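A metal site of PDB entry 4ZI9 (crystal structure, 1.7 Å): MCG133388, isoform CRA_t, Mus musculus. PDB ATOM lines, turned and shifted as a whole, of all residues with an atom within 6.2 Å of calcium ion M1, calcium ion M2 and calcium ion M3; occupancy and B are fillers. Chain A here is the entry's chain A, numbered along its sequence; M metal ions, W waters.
Calcium ion M1 is bound by OD1 of Asp 64 (2.2 Å), OE1 of Glu 66 (2.4 Å), OE1 of Glu 10 (2.4 Å), OD2 of Asp 101 (2.4 Å), OE2 of Glu 11 (2.5 Å) and water W1 (2.5 Å).
Calcium ion M1 has six donor atoms within binding distance.
Within 4 Å of calcium ion M3: Asn 100, Asn 102, Asp 132, Asp 134, Asn 138 and Asp 189.
Within 4 Å of calcium ion M1: Glu 10, Glu 11, Asp 64, Glu 66 and Asp 101.
The nearest printed residue that does not touch calcium ion M1 is Arg 65 (4.3 Å).
Calcium ion M3 is bound by OD1 of Asn 100, O of Asn 102, OD2 of Asp 189, O of Asn 138, OD2 of Asp 134, OD2 of Asp 132 and OD1 of Asp 132.
Calcium ion M3 has seven donor atoms within binding distance.
Calcium ion M2 is bound by OE2 of Glu 66 (2.3 Å), OD1 of Asp 101 (2.4 Å), OE2 of Glu 10 (2.4 Å), OD1 of Asp 134 (2.4 Å), O of Ile 99 (2.4 Å), OD1 of Asp 98 (2.5 Å) and OE1 of Glu 66 (2.5 Å).
Calcium ion M2 has seven donor atoms within binding distance.
The side-chain carboxylate (OD2) of Asp 98 sits at hydrogen-bond distance from the backbone NH (N) of Val 135.
The backbone NH (N) of Asp 189 is in hydrogen-bond range of the backbone carbonyl oxygen (O) of His 195, 2.9 Å away.
The backbone carbonyl oxygen of Asn 102 lies close to a ring nitrogen (ND1) of His 195 (3.5 Å).
The side-chain amide nitrogen (ND2) of Asn 138 is in hydrogen-bond range of the side-chain carboxylate (OD2) of Asp 98 (2.9 Å).
NE of Arg 62 lies within salt-bridge range of OE1 of Glu 11, 2.7 Å away.
NE of Arg 65 lies close to OD1 of Asp 98 (2.9 Å).
OD1 of Asp 101 lies close to ND2 of Asn 102.
The backbone carbonyl oxygen (O) of Ile 63 sits at hydrogen-bond distance from the backbone NH (N) of Glu 11 (2.7 Å).
Of the 26 residues printed, 7 come within 4 Å of calcium ion M2.
The nearest printed residue that does not touch calcium ion M2 is Arg 65 (4.4 Å).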
ATOM      1  N   GLU A  10     -15.902  20.090  -9.226  1.00  0.00           N
ATOM      2  CA  GLU A  10     -15.126  21.322  -9.184  1.00  0.00           C
ATOM      3  C   GLU A  10     -13.764  21.113  -9.866  1.00  0.00           C
ATOM      4  O   GLU A  10     -13.318  19.992 -10.052  1.00  0.00           O
ATOM      5  CB  GLU A  10     -14.907  21.752  -7.733  1.00  0.00           C
ATOM      6  CG  GLU A  10     -14.235  20.642  -6.960  1.00  0.00           C
ATOM      7  CD  GLU A  10     -13.726  21.069  -5.605  1.00  0.00           C
ATOM      8  OE1 GLU A  10     -13.392  22.259  -5.420  1.00  0.00           O
ATOM      9  OE2 GLU A  10     -13.660  20.197  -4.719  1.00  0.00           O
ATOM     10  N   GLU A  11     -13.133  22.220 -10.239  1.00  0.00           N
ATOM     11  CA  GLU A  11     -11.759  22.267 -10.754  1.00  0.00           C
ATOM     12  C   GLU A  11     -11.516  21.567 -12.102  1.00  0.00           C
ATOM     13  O   GLU A  11     -10.385  21.264 -12.441  1.00  0.00           O
ATOM     14  CB  GLU A  11     -10.781  21.689  -9.691  1.00  0.00           C
ATOM     15  CG  GLU A  11     -11.013  22.210  -8.250  1.00  0.00           C
ATOM     16  CD  GLU A  11     -10.576  23.649  -8.019  1.00  0.00           C
ATOM     17  OE1 GLU A  11     -10.153  24.319  -8.984  1.00  0.00           O
ATOM     18  OE2 GLU A  11     -10.639  24.104  -6.854  1.00  0.00           O
ATOM     19  N   ARG A  62     -12.830  28.857 -13.652  1.00  0.00           N
ATOM     20  CA  ARG A  62     -12.502  27.983 -12.534  1.00  0.00           C
ATOM     21  C   ARG A  62     -13.728  27.834 -11.628  1.00  0.00           C
ATOM     22  O   ARG A  62     -14.298  28.820 -11.187  1.00  0.00           O
ATOM     23  CB  ARG A  62     -11.310  28.501 -11.711  1.00  0.00           C
ATOM     24  CG  ARG A  62     -10.871  27.490 -10.647  1.00  0.00           C
ATOM     25  CD  ARG A  62      -9.794  27.987  -9.656  1.00  0.00           C
ATOM     26  NE  ARG A  62      -9.591  26.979  -8.618  1.00  0.00           N
ATOM     27  CZ  ARG A  62      -9.028  27.198  -7.429  1.00  0.00           C
ATOM     28  NH1 ARG A  62      -8.581  28.415  -7.108  1.00  0.00           N
ATOM     29  NH2 ARG A  62      -8.901  26.222  -6.541  1.00  0.00           N
ATOM     30  N   ILE A  63     -14.144  26.598 -11.379  1.00  0.00           N
ATOM     31  CA  ILE A  63     -15.176  26.355 -10.373  1.00  0.00           C
ATOM     32  C   ILE A  63     -14.547  25.685  -9.142  1.00  0.00           C
ATOM     33  O   ILE A  63     -14.141  24.517  -9.183  1.00  0.00           O
ATOM     34  CB  ILE A  63     -16.335  25.488 -10.936  1.00  0.00           C
ATOM     35  CG1 ILE A  63     -16.805  26.043 -12.291  1.00  0.00           C
ATOM     36  CG2 ILE A  63     -17.482  25.445  -9.915  1.00  0.00           C
ATOM     37  CD1 ILE A  63     -17.897  25.238 -12.967  1.00  0.00           C
ATOM     38  N   ASP A  64     -14.450  26.444  -8.053  1.00  0.00           N
ATOM     39  CA  ASP A  64     -13.875  25.945  -6.810  1.00  0.00           C
ATOM     40  C   ASP A  64     -14.976  25.817  -5.766  1.00  0.00           C
ATOM     41  O   ASP A  64     -15.479  26.816  -5.269  1.00  0.00           O
ATOM     42  CB  ASP A  64     -12.771  26.881  -6.314  1.00  0.00           C
ATOM     43  CG  ASP A  64     -12.244  26.519  -4.915  1.00  0.00           C
ATOM     44  OD1 ASP A  64     -12.294  25.333  -4.501  1.00  0.00           O
ATOM     45  OD2 ASP A  64     -11.788  27.439  -4.211  1.00  0.00           O
ATOM     46  N   ARG A  65     -15.354  24.578  -5.434  1.00  0.00           N
ATOM     47  CA  ARG A  65     -16.424  24.313  -4.466  1.00  0.00           C
ATOM     48  C   ARG A  65     -16.141  24.933  -3.103  1.00  0.00           C
ATOM     49  O   ARG A  65     -17.051  25.372  -2.403  1.00  0.00           O
ATOM     50  CB  ARG A  65     -16.660  22.802  -4.311  1.00  0.00           C
ATOM     51  CG  ARG A  65     -17.975  22.476  -3.579  1.00  0.00           C
ATOM     52  CD  ARG A  65     -17.859  21.214  -2.769  1.00  0.00           C
ATOM     53  NE  ARG A  65     -16.847  21.395  -1.724  1.00  0.00           N
ATOM     54  CZ  ARG A  65     -17.052  22.072  -0.608  1.00  0.00           C
ATOM     55  NH1 ARG A  65     -18.239  22.617  -0.364  1.00  0.00           N
ATOM     56  NH2 ARG A  65     -16.053  22.208   0.267  1.00  0.00           N
ATOM     57  N   GLU A  66     -14.873  24.964  -2.727  1.00  0.00           N
ATOM     58  CA  GLU A  66     -14.524  25.520  -1.430  1.00  0.00           C
ATOM     59  C   GLU A  66     -14.861  27.011  -1.399  1.00  0.00           C
ATOM     60  O   GLU A  66     -15.479  27.491  -0.457  1.00  0.00           O
ATOM     61  CB  GLU A  66     -13.040  25.278  -1.110  1.00  0.00           C
ATOM     62  CG  GLU A  66     -12.752  23.888  -0.537  1.00  0.00           C
ATOM     63  CD  GLU A  66     -12.923  22.737  -1.518  1.00  0.00           C
ATOM     64  OE1 GLU A  66     -12.238  22.666  -2.551  1.00  0.00           O
ATOM     65  OE2 GLU A  66     -13.722  21.828  -1.215  1.00  0.00           O
ATOM     66  N   GLU A  67     -14.500  27.726  -2.462  1.00  0.00           N
ATOM     67  CA  GLU A  67     -14.819  29.147  -2.529  1.00  0.00           C
ATOM     68  C   GLU A  67     -16.326  29.422  -2.578  1.00  0.00           C
ATOM     69  O   GLU A  67     -16.806  30.385  -1.971  1.00  0.00           O
ATOM     70  CB  GLU A  67     -14.150  29.787  -3.741  1.00  0.00           C
ATOM     71  CG  GLU A  67     -14.462  31.272  -3.875  1.00  0.00           C
ATOM     72  CD  GLU A  67     -14.050  31.839  -5.224  1.00  0.00           C
ATOM     73  OE1 GLU A  67     -13.127  31.272  -5.851  1.00  0.00           O
ATOM     74  OE2 GLU A  67     -14.661  32.843  -5.660  1.00  0.00           O
ATOM     75  N   ASP A  98     -17.757  17.857  -4.792  1.00  0.00           N
ATOM     76  CA  ASP A  98     -16.509  18.067  -4.064  1.00  0.00           C
ATOM     77  C   ASP A  98     -15.453  17.089  -4.528  1.00  0.00           C
ATOM     78  O   ASP A  98     -15.742  15.912  -4.715  1.00  0.00           O
ATOM     79  CB  ASP A  98     -16.732  17.896  -2.555  1.00  0.00           C
ATOM     80  CG  ASP A  98     -15.491  18.180  -1.736  1.00  0.00           C
ATOM     81  OD1 ASP A  98     -14.855  19.236  -1.931  1.00  0.00           O
ATOM     82  OD2 ASP A  98     -15.168  17.360  -0.841  1.00  0.00           O
ATOM     83  N   ILE A  99     -14.228  17.554  -4.734  1.00  0.00           N
ATOM     84  CA  ILE A  99     -13.144  16.605  -4.887  1.00  0.00           C
ATOM     85  C   ILE A  99     -12.197  16.835  -3.719  1.00  0.00           C
ATOM     86  O   ILE A  99     -12.239  17.877  -3.044  1.00  0.00           O
ATOM     87  CB  ILE A  99     -12.377  16.761  -6.200  1.00  0.00           C
ATOM     88  CG1 ILE A  99     -11.536  18.028  -6.170  1.00  0.00           C
ATOM     89  CG2 ILE A  99     -13.352  16.772  -7.398  1.00  0.00           C
ATOM     90  CD1 ILE A  99     -10.614  18.167  -7.365  1.00  0.00           C
ATOM     91  N   ASN A 100     -11.344  15.852  -3.501  1.00  0.00           N
ATOM     92  CA  ASN A 100     -10.432  15.925  -2.375  1.00  0.00           C
ATOM     93  C   ASN A 100      -9.183  16.673  -2.753  1.00  0.00           C
ATOM     94  O   ASN A 100      -8.134  16.058  -2.924  1.00  0.00           O
ATOM     95  CB  ASN A 100     -10.080  14.514  -1.887  1.00  0.00           C
ATOM     96  CG  ASN A 100      -9.454  14.549  -0.496  1.00  0.00           C
ATOM     97  OD1 ASN A 100      -9.752  15.455   0.266  1.00  0.00           O
ATOM     98  ND2 ASN A 100      -8.612  13.576  -0.179  1.00  0.00           N
ATOM     99  N   ASP A 101      -9.262  17.999  -2.872  1.00  0.00           N
ATOM    100  CA  ASP A 101      -8.092  18.781  -3.260  1.00  0.00           C
ATOM    101  C   ASP A 101      -7.535  19.641  -2.111  1.00  0.00           C
ATOM    102  O   ASP A 101      -6.843  20.632  -2.345  1.00  0.00           O
ATOM    103  CB  ASP A 101      -8.395  19.684  -4.470  1.00  0.00           C
ATOM    104  CG  ASP A 101      -9.674  20.499  -4.322  1.00  0.00           C
ATOM    105  OD1 ASP A 101     -10.523  20.136  -3.478  1.00  0.00           O
ATOM    106  OD2 ASP A 101      -9.848  21.488  -5.066  1.00  0.00           O
ATOM    107  N   ASN A 102      -7.880  19.267  -0.887  1.00  0.00           N
ATOM    108  CA  ASN A 102      -7.353  19.965   0.276  1.00  0.00           C
ATOM    109  C   ASN A 102      -6.856  18.965   1.297  1.00  0.00           C
ATOM    110  O   ASN A 102      -7.456  17.913   1.483  1.00  0.00           O
ATOM    111  CB  ASN A 102      -8.399  20.876   0.900  1.00  0.00           C
ATOM    112  CG  ASN A 102      -8.715  22.062   0.024  1.00  0.00           C
ATOM    113  OD1 ASN A 102      -8.030  23.093   0.076  1.00  0.00           O
ATOM    114  ND2 ASN A 102      -9.753  21.931  -0.793  1.00  0.00           N
ATOM    115  N   THR A 103      -5.720  19.285   1.914  1.00  0.00           N
ATOM    116  CA  THR A 103      -5.160  18.502   3.011  1.00  0.00           C
ATOM    117  C   THR A 103      -5.540  19.129   4.350  1.00  0.00           C
ATOM    118  O   THR A 103      -5.539  20.371   4.477  1.00  0.00           O
ATOM    119  CB  THR A 103      -3.633  18.418   2.859  1.00  0.00           C
ATOM    120  OG1 THR A 103      -3.322  17.803   1.607  1.00  0.00           O
ATOM    121  CG2 THR A 103      -2.985  17.638   4.011  1.00  0.00           C
ATOM    122  N   PRO A 104      -5.857  18.309   5.368  1.00  0.00           N
ATOM    123  CA  PRO A 104      -6.096  18.903   6.692  1.00  0.00           C
ATOM    124  C   PRO A 104      -4.916  19.785   7.128  1.00  0.00           C
ATOM    125  O   PRO A 104      -3.767  19.391   7.024  1.00  0.00           O
ATOM    126  CB  PRO A 104      -6.244  17.679   7.610  1.00  0.00           C
ATOM    127  CG  PRO A 104      -6.677  16.582   6.703  1.00  0.00           C
ATOM    128  CD  PRO A 104      -6.016  16.840   5.379  1.00  0.00           C
ATOM    129  N   ASP A 132      -9.912  20.622   7.565  1.00  0.00           N
ATOM    130  CA  ASP A 132      -9.918  20.289   6.139  1.00  0.00           C
ATOM    131  C   ASP A 132     -11.009  21.072   5.402  1.00  0.00           C
ATOM    132  O   ASP A 132     -12.169  21.030   5.795  1.00  0.00           O
ATOM    133  CB  ASP A 132     -10.151  18.781   5.981  1.00  0.00           C
ATOM    134  CG  ASP A 132      -9.807  18.262   4.592  1.00  0.00           C
ATOM    135  OD1 ASP A 132     -10.318  18.803   3.583  1.00  0.00           O
ATOM    136  OD2 ASP A 132      -9.021  17.313   4.505  1.00  0.00           O
ATOM    137  N   LEU A 133     -10.643  21.809   4.349  1.00  0.00           N
ATOM    138  CA  LEU A 133     -11.589  22.661   3.617  1.00  0.00           C
ATOM    139  C   LEU A 133     -12.601  21.893   2.783  1.00  0.00           C
ATOM    140  O   LEU A 133     -13.635  22.438   2.373  1.00  0.00           O
ATOM    141  CB  LEU A 133     -10.844  23.628   2.716  1.00  0.00           C
ATOM    142  CG  LEU A 133      -9.993  24.654   3.458  1.00  0.00           C
ATOM    143  CD1 LEU A 133      -9.295  25.571   2.463  1.00  0.00           C
ATOM    144  CD2 LEU A 133     -10.868  25.453   4.413  1.00  0.00           C
ATOM    145  N   ASP A 134     -12.294  20.630   2.502  1.00  0.00           N
ATOM    146  CA  ASP A 134     -13.221  19.782   1.750  1.00  0.00           C
ATOM    147  C   ASP A 134     -14.420  19.415   2.621  1.00  0.00           C
ATOM    148  O   ASP A 134     -14.539  19.859   3.770  1.00  0.00           O
ATOM    149  CB  ASP A 134     -12.509  18.542   1.240  1.00  0.00           C
ATOM    150  CG  ASP A 134     -11.342  18.885   0.339  1.00  0.00           C
ATOM    151  OD1 ASP A 134     -11.458  19.825  -0.477  1.00  0.00           O
ATOM    152  OD2 ASP A 134     -10.305  18.196   0.422  1.00  0.00           O
ATOM    153  N   VAL A 135     -15.351  18.636   2.075  1.00  0.00           N
ATOM    154  CA  VAL A 135     -16.525  18.261   2.826  1.00  0.00           C
ATOM    155  C   VAL A 135     -16.743  16.765   2.788  1.00  0.00           C
ATOM    156  O   VAL A 135     -16.117  16.061   1.995  1.00  0.00           O
ATOM    157  CB  VAL A 135     -17.789  18.959   2.307  1.00  0.00           C
ATOM    158  CG1 VAL A 135     -17.723  20.438   2.639  1.00  0.00           C
ATOM    159  CG2 VAL A 135     -17.936  18.742   0.800  1.00  0.00           C
ATOM    160  N   ASN A 138     -14.223  13.665   2.365  1.00  0.00           N
ATOM    161  CA  ASN A 138     -12.969  14.332   2.046  1.00  0.00           C
ATOM    162  C   ASN A 138     -12.493  15.245   3.165  1.00  0.00           C
ATOM    163  O   ASN A 138     -11.416  15.850   3.056  1.00  0.00           O
ATOM    164  CB  ASN A 138     -13.102  15.121   0.751  1.00  0.00           C
ATOM    165  CG  ASN A 138     -13.358  14.231  -0.434  1.00  0.00           C
ATOM    166  OD1 ASN A 138     -12.846  13.102  -0.485  1.00  0.00           O
ATOM    167  ND2 ASN A 138     -14.167  14.707  -1.383  1.00  0.00           N
ATOM    168  N   SER A 139     -13.273  15.374   4.223  1.00  0.00           N
ATOM    169  CA  SER A 139     -12.802  16.180   5.347  1.00  0.00           C
ATOM    170  C   SER A 139     -12.091  15.321   6.397  1.00  0.00           C
ATOM    171  O   SER A 139     -11.895  14.105   6.229  1.00  0.00           O
ATOM    172  CB  SER A 139     -13.964  16.967   5.979  1.00  0.00           C
ATOM    173  OG  SER A 139     -15.020  16.105   6.329  1.00  0.00           O
ATOM    174  N   LEU A 140     -11.700  15.979   7.483  1.00  0.00           N
ATOM    175  CA  LEU A 140     -10.938  15.346   8.560  1.00  0.00           C
ATOM    176  C   LEU A 140     -11.638  14.078   9.050  1.00  0.00           C
ATOM    177  O   LEU A 140     -12.817  14.110   9.368  1.00  0.00           O
ATOM    178  CB  LEU A 140     -10.758  16.321   9.715  1.00  0.00           C
ATOM    179  CG  LEU A 140      -9.940  15.828  10.923  1.00  0.00           C
ATOM    180  CD1 LEU A 140      -8.528  15.553  10.507  1.00  0.00           C
ATOM    181  CD2 LEU A 140      -9.964  16.866  12.027  1.00  0.00           C
ATOM    182  N   ASP A 189      -7.542  12.933   6.106  1.00  0.00           N
ATOM    183  CA  ASP A 189      -8.936  12.965   5.703  1.00  0.00           C
ATOM    184  C   ASP A 189      -9.332  11.560   5.255  1.00  0.00           C
ATOM    185  O   ASP A 189      -8.575  10.617   5.451  1.00  0.00           O
ATOM    186  CB  ASP A 189      -9.190  14.007   4.594  1.00  0.00           C
ATOM    187  CG  ASP A 189      -8.358  13.786   3.324  1.00  0.00           C
ATOM    188  OD1 ASP A 189      -7.983  12.631   3.013  1.00  0.00           O
ATOM    189  OD2 ASP A 189      -8.110  14.789   2.617  1.00  0.00           O
ATOM    190  N   GLY A 190     -10.502  11.411   4.639  1.00  0.00           N
ATOM    191  CA  GLY A 190     -10.937  10.089   4.244  1.00  0.00           C
ATOM    192  C   GLY A 190     -10.998   9.856   2.744  1.00  0.00           C
ATOM    193  O   GLY A 190     -11.731   8.987   2.261  1.00  0.00           O
ATOM    194  N   GLY A 191     -10.209  10.627   1.984  1.00  0.00           N
ATOM    195  CA  GLY A 191     -10.185  10.488   0.536  1.00  0.00           C
ATOM    196  C   GLY A 191      -9.410   9.247   0.128  1.00  0.00           C
ATOM    197  O   GLY A 191      -8.968   8.477   0.981  1.00  0.00           O
ATOM    198  N   HIS A 195      -5.143  12.255   2.280  1.00  0.00           N
ATOM    199  CA  HIS A 195      -4.245  13.378   2.531  1.00  0.00           C
ATOM    200  C   HIS A 195      -4.038  13.499   4.030  1.00  0.00           C
ATOM    201  O   HIS A 195      -4.988  13.333   4.788  1.00  0.00           O
ATOM    202  CB  HIS A 195      -4.814  14.678   1.983  1.00  0.00           C
ATOM    203  CG  HIS A 195      -4.883  14.705   0.489  1.00  0.00           C
ATOM    204  ND1 HIS A 195      -5.282  15.813  -0.220  1.00  0.00           N
ATOM    205  CD2 HIS A 195      -4.593  13.745  -0.425  1.00  0.00           C
ATOM    206  CE1 HIS A 195      -5.249  15.539  -1.512  1.00  0.00           C
ATOM    207  NE2 HIS A 195      -4.839  14.295  -1.666  1.00  0.00           N
HETATM  208 CA    CA M   1     -11.373  23.292  -4.651  1.00  0.00          CA
HETATM  209 CA    CA M   2     -12.689  20.220  -2.533  1.00  0.00          CA
HETATM  210 CA    CA M   3      -9.384  16.744   2.152  1.00  0.00          CA
HETATM  211  O   HOH W   1      -9.305  24.067  -3.426  1.00  0.00           O
